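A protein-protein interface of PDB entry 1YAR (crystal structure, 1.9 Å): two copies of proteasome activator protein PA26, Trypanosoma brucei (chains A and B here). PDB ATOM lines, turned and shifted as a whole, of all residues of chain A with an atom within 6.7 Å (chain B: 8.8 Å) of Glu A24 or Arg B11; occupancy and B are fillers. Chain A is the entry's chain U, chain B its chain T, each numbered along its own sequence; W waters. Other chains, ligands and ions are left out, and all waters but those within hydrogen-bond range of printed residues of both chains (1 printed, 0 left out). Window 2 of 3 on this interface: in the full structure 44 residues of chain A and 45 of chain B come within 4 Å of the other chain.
The guanidinium group of Arg B11 lies within salt-bridge range of the side-chain carboxylate of Glu A24 (2.8 Å). The indole nitrogen (NE1) of Trp A222 lies close to the guanidinium group (NH1) of Arg B11.
O of Glu A24 lies within hydrogen-bond range of OG of Ser A27. OE1 of Glu A24 sits at hydrogen-bond distance from OH of Tyr A218 (2.4 Å).
Among the printed residues, merely in contact across the chains: Leu A219 with Leu B14 (3.6 Å), Leu A219 with Ile B15 (3.7 Å), Phe A28 with Arg B11 (3.8 Å), Leu A219 with Arg B11 (3.9 Å) and Phe A28 with Leu B14 (3.9 Å).
Thr A23 touches none of the printed residues of chain B. Of chain B, only Arg B11 comes within 4 Å of Glu A24. Printed residues of chain B within 4 Å of Phe A28: Arg B11 and Leu B14. Val A97 touches none of the printed residues of chain B. Tyr A218 touches none of the printed residues of chain B. Of the printed residues of chain B, Trp A222 touches Arg B11. Arg B11 touches just these residues of chain A: Glu A24 (2.8 Å), Phe A28 (3.8 Å), Leu A219 (3.9 Å) and Trp A222 (3.3 Å). Printed residues of chain A within 4 Å of Leu B14: Phe A28 (3.9 Å) and Leu A219 (3.6 Å). Of the printed residues of chain A, Ile B15 touches Leu A219. The nearest printed residue of chain B that does not touch Glu A24 is Leu B14 (9.1 Å). The nearest printed residue of chain A that does not touch Leu B14 is Tyr A218 (7.7 Å).
Printed residues of chain A that touch a printed residue of chain B: Glu A24, Phe A28, Leu A219 and Trp A222. Hydrophobic or aromatic side chains of chain A that line the printed part of chain B: Phe A28, Leu A219 and Trp A222. Of the 9 printed residues of chain B, 3 touch a printed residue of chain A.
No position is printed for both chains.
Water W1 lies within hydrogen-bond range of the side-chain carboxylate of Glu A24, the side-chain hydroxyl of Thr A25 and the guanidinium group of Arg B11.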
ATOM      1  N   ARG A  19      18.373   7.255  -4.042  1.00  0.00           N
ATOM      2  CA  ARG A  19      18.816   7.923  -5.256  1.00  0.00           C
ATOM      3  C   ARG A  19      18.077   9.236  -5.551  1.00  0.00           C
ATOM      4  O   ARG A  19      18.665  10.173  -6.100  1.00  0.00           O
ATOM      5  CB  ARG A  19      18.736   6.968  -6.450  1.00  0.00           C
ATOM      6  CG  ARG A  19      19.750   5.832  -6.348  1.00  0.00           C
ATOM      7  CD  ARG A  19      19.773   4.898  -7.546  1.00  0.00           C
ATOM      8  NE  ARG A  19      20.611   3.732  -7.260  1.00  0.00           N
ATOM      9  CZ  ARG A  19      20.641   2.636  -8.002  1.00  0.00           C
ATOM     10  NH1 ARG A  19      19.857   2.546  -9.069  1.00  0.00           N
ATOM     11  NH2 ARG A  19      21.428   1.618  -7.653  1.00  0.00           N
ATOM     12  N   TYR A  22      19.790  12.010  -3.226  1.00  0.00           N
ATOM     13  CA  TYR A  22      21.125  12.453  -3.645  1.00  0.00           C
ATOM     14  C   TYR A  22      21.241  12.239  -5.123  1.00  0.00           C
ATOM     15  O   TYR A  22      21.606  11.153  -5.544  1.00  0.00           O
ATOM     16  CB  TYR A  22      22.202  11.629  -2.923  1.00  0.00           C
ATOM     17  CG  TYR A  22      22.329  12.058  -1.494  1.00  0.00           C
ATOM     18  CD1 TYR A  22      21.505  11.514  -0.506  1.00  0.00           C
ATOM     19  CD2 TYR A  22      23.226  13.058  -1.140  1.00  0.00           C
ATOM     20  CE1 TYR A  22      21.589  11.945   0.813  1.00  0.00           C
ATOM     21  CE2 TYR A  22      23.333  13.486   0.178  1.00  0.00           C
ATOM     22  CZ  TYR A  22      22.504  12.931   1.138  1.00  0.00           C
ATOM     23  OH  TYR A  22      22.618  13.370   2.434  1.00  0.00           O
ATOM     24  N   THR A  23      20.901  13.261  -5.911  1.00  0.00           N
ATOM     25  CA  THR A  23      20.826  13.116  -7.358  1.00  0.00           C
ATOM     26  C   THR A  23      22.041  13.751  -8.008  1.00  0.00           C
ATOM     27  O   THR A  23      22.861  14.383  -7.325  1.00  0.00           O
ATOM     28  CB  THR A  23      19.585  13.835  -7.909  1.00  0.00           C
ATOM     29  OG1 THR A  23      19.776  15.232  -7.682  1.00  0.00           O
ATOM     30  CG2 THR A  23      18.306  13.472  -7.138  1.00  0.00           C
ATOM     31  N   GLU A  24      22.135  13.625  -9.333  1.00  0.00           N
ATOM     32  CA  GLU A  24      23.218  14.290 -10.090  1.00  0.00           C
ATOM     33  C   GLU A  24      23.210  15.814  -9.851  1.00  0.00           C
ATOM     34  O   GLU A  24      24.268  16.462  -9.846  1.00  0.00           O
ATOM     35  CB  GLU A  24      23.117  13.977 -11.580  1.00  0.00           C
ATOM     36  CG  GLU A  24      24.406  14.228 -12.383  1.00  0.00           C
ATOM     37  CD  GLU A  24      24.629  15.690 -12.772  1.00  0.00           C
ATOM     38  OE1 GLU A  24      25.789  16.179 -12.686  1.00  0.00           O
ATOM     39  OE2 GLU A  24      23.657  16.367 -13.184  1.00  0.00           O
ATOM     40  N   THR A  25      22.019  16.383  -9.638  1.00  0.00           N
ATOM     41  CA  THR A  25      21.943  17.805  -9.317  1.00  0.00           C
ATOM     42  C   THR A  25      22.684  18.135  -8.022  1.00  0.00           C
ATOM     43  O   THR A  25      23.350  19.170  -7.948  1.00  0.00           O
ATOM     44  CB  THR A  25      20.492  18.301  -9.258  1.00  0.00           C
ATOM     45  OG1 THR A  25      19.852  18.023 -10.511  1.00  0.00           O
ATOM     46  CG2 THR A  25      20.489  19.815  -9.223  1.00  0.00           C
ATOM     47  N   SER A  26      22.590  17.260  -7.024  1.00  0.00           N
ATOM     48  CA  SER A  26      23.296  17.474  -5.755  1.00  0.00           C
ATOM     49  C   SER A  26      24.804  17.542  -5.952  1.00  0.00           C
ATOM     50  O   SER A  26      25.475  18.391  -5.357  1.00  0.00           O
ATOM     51  CB  SER A  26      23.017  16.365  -4.740  1.00  0.00           C
ATOM     52  OG  SER A  26      21.641  16.070  -4.629  1.00  0.00           O
ATOM     53  N   SER A  27      25.335  16.629  -6.761  1.00  0.00           N
ATOM     54  CA  SER A  27      26.797  16.593  -6.979  1.00  0.00           C
ATOM     55  C   SER A  27      27.239  17.714  -7.894  1.00  0.00           C
ATOM     56  O   SER A  27      28.257  18.364  -7.630  1.00  0.00           O
ATOM     57  CB  SER A  27      27.231  15.228  -7.527  1.00  0.00           C
ATOM     58  OG  SER A  27      26.356  14.784  -8.548  1.00  0.00           O
ATOM     59  N   PHE A  28      26.450  17.980  -8.945  1.00  0.00           N
ATOM     60  CA  PHE A  28      26.714  19.110  -9.826  1.00  0.00           C
ATOM     61  C   PHE A  28      26.753  20.450  -9.089  1.00  0.00           C
ATOM     62  O   PHE A  28      27.590  21.296  -9.383  1.00  0.00           O
ATOM     63  CB  PHE A  28      25.721  19.168 -10.998  1.00  0.00           C
ATOM     64  CG  PHE A  28      26.060  20.224 -12.027  1.00  0.00           C
ATOM     65  CD1 PHE A  28      27.285  20.217 -12.680  1.00  0.00           C
ATOM     66  CD2 PHE A  28      25.151  21.244 -12.322  1.00  0.00           C
ATOM     67  CE1 PHE A  28      27.614  21.205 -13.631  1.00  0.00           C
ATOM     68  CE2 PHE A  28      25.449  22.237 -13.282  1.00  0.00           C
ATOM     69  CZ  PHE A  28      26.693  22.217 -13.942  1.00  0.00           C
ATOM     70  N   ALA A  29      25.834  20.637  -8.140  1.00  0.00           N
ATOM     71  CA  ALA A  29      25.796  21.868  -7.362  1.00  0.00           C
ATOM     72  C   ALA A  29      27.102  22.063  -6.584  1.00  0.00           C
ATOM     73  O   ALA A  29      27.606  23.191  -6.453  1.00  0.00           O
ATOM     74  CB  ALA A  29      24.604  21.865  -6.433  1.00  0.00           C
ATOM     75  N   VAL A  97      26.487  10.394  -3.989  1.00  0.00           N
ATOM     76  CA  VAL A  97      25.785  10.334  -5.282  1.00  0.00           C
ATOM     77  C   VAL A  97      26.319   9.150  -6.116  1.00  0.00           C
ATOM     78  O   VAL A  97      25.548   8.397  -6.721  1.00  0.00           O
ATOM     79  CB  VAL A  97      25.929  11.653  -6.061  1.00  0.00           C
ATOM     80  CG1 VAL A  97      25.443  11.489  -7.510  1.00  0.00           C
ATOM     81  CG2 VAL A  97      25.153  12.803  -5.372  1.00  0.00           C
ATOM     82  N   ARG A 101      24.955   4.460  -6.590  1.00  0.00           N
ATOM     83  CA  ARG A 101      24.684   4.063  -7.976  1.00  0.00           C
ATOM     84  C   ARG A 101      25.700   3.027  -8.519  1.00  0.00           C
ATOM     85  O   ARG A 101      25.649   2.671  -9.703  1.00  0.00           O
ATOM     86  CB  ARG A 101      24.628   5.296  -8.886  1.00  0.00           C
ATOM     87  CG  ARG A 101      23.409   6.200  -8.578  1.00  0.00           C
ATOM     88  CD  ARG A 101      23.352   7.458  -9.411  1.00  0.00           C
ATOM     89  NE  ARG A 101      22.084   8.173  -9.197  1.00  0.00           N
ATOM     90  CZ  ARG A 101      21.793   8.912  -8.128  1.00  0.00           C
ATOM     91  NH1 ARG A 101      22.681   9.061  -7.141  1.00  0.00           N
ATOM     92  NH2 ARG A 101      20.599   9.513  -8.043  1.00  0.00           N
ATOM     93  N   TYR A 218      34.901  15.074 -12.743  1.00  0.00           N
ATOM     94  CA  TYR A 218      33.435  14.984 -12.640  1.00  0.00           C
ATOM     95  C   TYR A 218      32.736  15.365 -13.959  1.00  0.00           C
ATOM     96  O   TYR A 218      31.886  14.599 -14.459  1.00  0.00           O
ATOM     97  CB  TYR A 218      32.896  15.816 -11.454  1.00  0.00           C
ATOM     98  CG  TYR A 218      31.394  15.664 -11.312  1.00  0.00           C
ATOM     99  CD1 TYR A 218      30.849  14.684 -10.462  1.00  0.00           C
ATOM    100  CD2 TYR A 218      30.516  16.457 -12.073  1.00  0.00           C
ATOM    101  CE1 TYR A 218      29.458  14.505 -10.372  1.00  0.00           C
ATOM    102  CE2 TYR A 218      29.132  16.292 -11.967  1.00  0.00           C
ATOM    103  CZ  TYR A 218      28.619  15.334 -11.110  1.00  0.00           C
ATOM    104  OH  TYR A 218      27.254  15.173 -11.002  1.00  0.00           O
ATOM    105  N   LEU A 219      33.099  16.516 -14.534  1.00  0.00           N
ATOM    106  CA  LEU A 219      32.381  17.034 -15.692  1.00  0.00           C
ATOM    107  C   LEU A 219      32.604  16.170 -16.934  1.00  0.00           C
ATOM    108  O   LEU A 219      31.727  16.061 -17.778  1.00  0.00           O
ATOM    109  CB  LEU A 219      32.751  18.497 -15.973  1.00  0.00           C
ATOM    110  CG  LEU A 219      32.254  19.434 -14.866  1.00  0.00           C
ATOM    111  CD1 LEU A 219      32.833  20.833 -15.063  1.00  0.00           C
ATOM    112  CD2 LEU A 219      30.711  19.472 -14.778  1.00  0.00           C
ATOM    113  N   TRP A 222      30.519  12.382 -15.767  1.00  0.00           N
ATOM    114  CA  TRP A 222      29.290  12.340 -14.953  1.00  0.00           C
ATOM    115  C   TRP A 222      28.224  11.393 -15.507  1.00  0.00           C
ATOM    116  O   TRP A 222      27.511  10.777 -14.726  1.00  0.00           O
ATOM    117  CB  TRP A 222      28.695  13.736 -14.688  1.00  0.00           C
ATOM    118  CG  TRP A 222      28.100  14.346 -15.886  1.00  0.00           C
ATOM    119  CD1 TRP A 222      28.740  15.104 -16.825  1.00  0.00           C
ATOM    120  CD2 TRP A 222      26.732  14.241 -16.313  1.00  0.00           C
ATOM    121  NE1 TRP A 222      27.863  15.460 -17.820  1.00  0.00           N
ATOM    122  CE2 TRP A 222      26.617  14.963 -17.518  1.00  0.00           C
ATOM    123  CE3 TRP A 222      25.594  13.591 -15.802  1.00  0.00           C
ATOM    124  CZ2 TRP A 222      25.407  15.058 -18.229  1.00  0.00           C
ATOM    125  CZ3 TRP A 222      24.376  13.698 -16.501  1.00  0.00           C
ATOM    126  CH2 TRP A 222      24.299  14.435 -17.695  1.00  0.00           C
ATOM    127  N   LYS A 223      28.145  11.243 -16.835  1.00  0.00           N
ATOM    128  CA  LYS A 223      27.107  10.355 -17.394  1.00  0.00           C
ATOM    129  C   LYS A 223      27.258   8.917 -16.913  1.00  0.00           C
ATOM    130  O   LYS A 223      26.268   8.299 -16.495  1.00  0.00           O
ATOM    131  CB  LYS A 223      27.035  10.444 -18.918  1.00  0.00           C
ATOM    132  CG  LYS A 223      26.554  11.806 -19.406  1.00  0.00           C
ATOM    133  CD  LYS A 223      26.346  11.833 -20.940  1.00  0.00           C
ATOM    134  CE  LYS A 223      25.564  13.082 -21.351  1.00  0.00           C
ATOM    135  NZ  LYS A 223      25.661  13.375 -22.836  1.00  0.00           N
ATOM    136  N   ILE A 226      26.521   8.339 -13.099  1.00  0.00           N
ATOM    137  CA  ILE A 226      25.084   8.143 -12.759  1.00  0.00           C
ATOM    138  C   ILE A 226      24.491   6.854 -13.342  1.00  0.00           C
ATOM    139  O   ILE A 226      23.679   6.194 -12.681  1.00  0.00           O
ATOM    140  CB  ILE A 226      24.252   9.369 -13.204  1.00  0.00           C
ATOM    141  CG1 ILE A 226      24.827  10.663 -12.591  1.00  0.00           C
ATOM    142  CG2 ILE A 226      22.727   9.176 -12.873  1.00  0.00           C
ATOM    143  CD1 ILE A 226      24.947  10.706 -11.063  1.00  0.00           C
ATOM    144  N   LYS B  10      26.678  25.688 -17.415  1.00  0.00           N
ATOM    145  CA  LYS B  10      27.008  24.912 -18.650  1.00  0.00           C
ATOM    146  C   LYS B  10      28.334  24.145 -18.459  1.00  0.00           C
ATOM    147  O   LYS B  10      29.369  24.748 -18.152  1.00  0.00           O
ATOM    148  CB  LYS B  10      27.128  25.842 -19.846  1.00  0.00           C
ATOM    149  CG  LYS B  10      27.105  25.159 -21.193  1.00  0.00           C
ATOM    150  CD  LYS B  10      25.669  24.936 -21.633  1.00  0.00           C
ATOM    151  CE  LYS B  10      25.507  25.178 -23.109  1.00  0.00           C
ATOM    152  NZ  LYS B  10      25.247  26.624 -23.374  1.00  0.00           N
ATOM    153  N   ARG B  11      28.290  22.825 -18.657  1.00  0.00           N
ATOM    154  CA  ARG B  11      29.406  21.956 -18.268  1.00  0.00           C
ATOM    155  C   ARG B  11      30.669  22.207 -19.112  1.00  0.00           C
ATOM    156  O   ARG B  11      31.767  22.348 -18.573  1.00  0.00           O
ATOM    157  CB  ARG B  11      28.975  20.494 -18.314  1.00  0.00           C
ATOM    158  CG  ARG B  11      27.868  20.193 -17.331  1.00  0.00           C
ATOM    159  CD  ARG B  11      27.192  18.854 -17.528  1.00  0.00           C
ATOM    160  NE  ARG B  11      25.946  18.842 -16.755  1.00  0.00           N
ATOM    161  CZ  ARG B  11      25.749  18.154 -15.637  1.00  0.00           C
ATOM    162  NH1 ARG B  11      26.699  17.366 -15.147  1.00  0.00           N
ATOM    163  NH2 ARG B  11      24.584  18.250 -15.010  1.00  0.00           N
ATOM    164  N   ALA B  12      30.503  22.285 -20.426  1.00  0.00           N
ATOM    165  CA  ALA B  12      31.629  22.550 -21.311  1.00  0.00           C
ATOM    166  C   ALA B  12      32.269  23.886 -20.966  1.00  0.00           C
ATOM    167  O   ALA B  12      33.491  24.019 -21.040  1.00  0.00           O
ATOM    168  CB  ALA B  12      31.194  22.513 -22.770  1.00  0.00           C
ATOM    169  N   ALA B  13      31.458  24.876 -20.580  1.00  0.00           N
ATOM    170  CA  ALA B  13      31.987  26.189 -20.235  1.00  0.00           C
ATOM    171  C   ALA B  13      32.803  26.152 -18.938  1.00  0.00           C
ATOM    172  O   ALA B  13      33.800  26.852 -18.831  1.00  0.00           O
ATOM    173  CB  ALA B  13      30.855  27.227 -20.141  1.00  0.00           C
ATOM    174  N   LEU B  14      32.393  25.324 -17.971  1.00  0.00           N
ATOM    175  CA  LEU B  14      33.169  25.162 -16.749  1.00  0.00           C
ATOM    176  C   LEU B  14      34.551  24.573 -17.067  1.00  0.00           C
ATOM    177  O   LEU B  14      35.553  25.037 -16.528  1.00  0.00           O
ATOM    178  CB  LEU B  14      32.434  24.319 -15.702  1.00  0.00           C
ATOM    179  CG  LEU B  14      31.167  24.912 -15.035  1.00  0.00           C
ATOM    180  CD1 LEU B  14      30.420  23.871 -14.209  1.00  0.00           C
ATOM    181  CD2 LEU B  14      31.472  26.132 -14.154  1.00  0.00           C
ATOM    182  N   ILE B  15      34.593  23.567 -17.947  1.00  0.00           N
ATOM    183  CA  ILE B  15      35.864  22.925 -18.338  1.00  0.00           C
ATOM    184  C   ILE B  15      36.711  23.920 -19.119  1.00  0.00           C
ATOM    185  O   ILE B  15      37.921  24.012 -18.921  1.00  0.00           O
ATOM    186  CB  ILE B  15      35.596  21.648 -19.191  1.00  0.00           C
ATOM    187  CG1 ILE B  15      35.043  20.521 -18.315  1.00  0.00           C
ATOM    188  CG2 ILE B  15      36.897  21.201 -19.935  1.00  0.00           C
ATOM    189  CD1 ILE B  15      34.486  19.362 -19.129  1.00  0.00           C
ATOM    190  N   GLN B  16      36.063  24.680 -20.001  1.00  0.00           N
ATOM    191  CA  GLN B  16      36.752  25.685 -20.816  1.00  0.00           C
ATOM    192  C   GLN B  16      37.388  26.794 -19.949  1.00  0.00           C
ATOM    193  O   GLN B  16      38.504  27.228 -20.226  1.00  0.00           O
ATOM    194  CB  GLN B  16      35.791  26.311 -21.835  1.00  0.00           C
ATOM    195  CG  GLN B  16      36.434  27.362 -22.752  1.00  0.00           C
ATOM    196  CD  GLN B  16      35.545  28.613 -22.963  1.00  0.00           C
ATOM    197  OE1 GLN B  16      34.329  28.597 -22.668  1.00  0.00           O
ATOM    198  NE2 GLN B  16      36.159  29.706 -23.447  1.00  0.00           N
ATOM    199  N   ASN B  17      36.673  27.270 -18.929  1.00  0.00           N
ATOM    200  CA  ASN B  17      37.256  28.235 -17.993  1.00  0.00           C
ATOM    201  C   ASN B  17      38.486  27.685 -17.257  1.00  0.00           C
ATOM    202  O   ASN B  17      39.482  28.397 -17.108  1.00  0.00           O
ATOM    203  CB  ASN B  17      36.234  28.737 -16.969  1.00  0.00           C
ATOM    204  CG  ASN B  17      36.868  29.687 -15.948  1.00  0.00           C
ATOM    205  OD1 ASN B  17      37.576  30.637 -16.325  1.00  0.00           O
ATOM    206  ND2 ASN B  17      36.661  29.414 -14.661  1.00  0.00           N
ATOM    207  N   LEU B  18      38.427  26.426 -16.800  1.00  0.00           N
ATOM    208  CA  LEU B  18      39.608  25.794 -16.162  1.00  0.00           C
ATOM    209  C   LEU B  18      40.800  25.820 -17.101  1.00  0.00           C
ATOM    210  O   LEU B  18      41.919  26.257 -16.765  1.00  0.00           O
ATOM    211  CB  LEU B  18      39.324  24.313 -15.810  1.00  0.00           C
ATOM    212  CG  LEU B  18      38.699  23.832 -14.515  1.00  0.00           C
ATOM    213  CD1 LEU B  18      38.711  22.294 -14.458  1.00  0.00           C
ATOM    214  CD2 LEU B  18      39.432  24.403 -13.300  1.00  0.00           C
HETATM  215  O   HOH W   1      22.161  18.592 -12.709  1.00  0.00           O
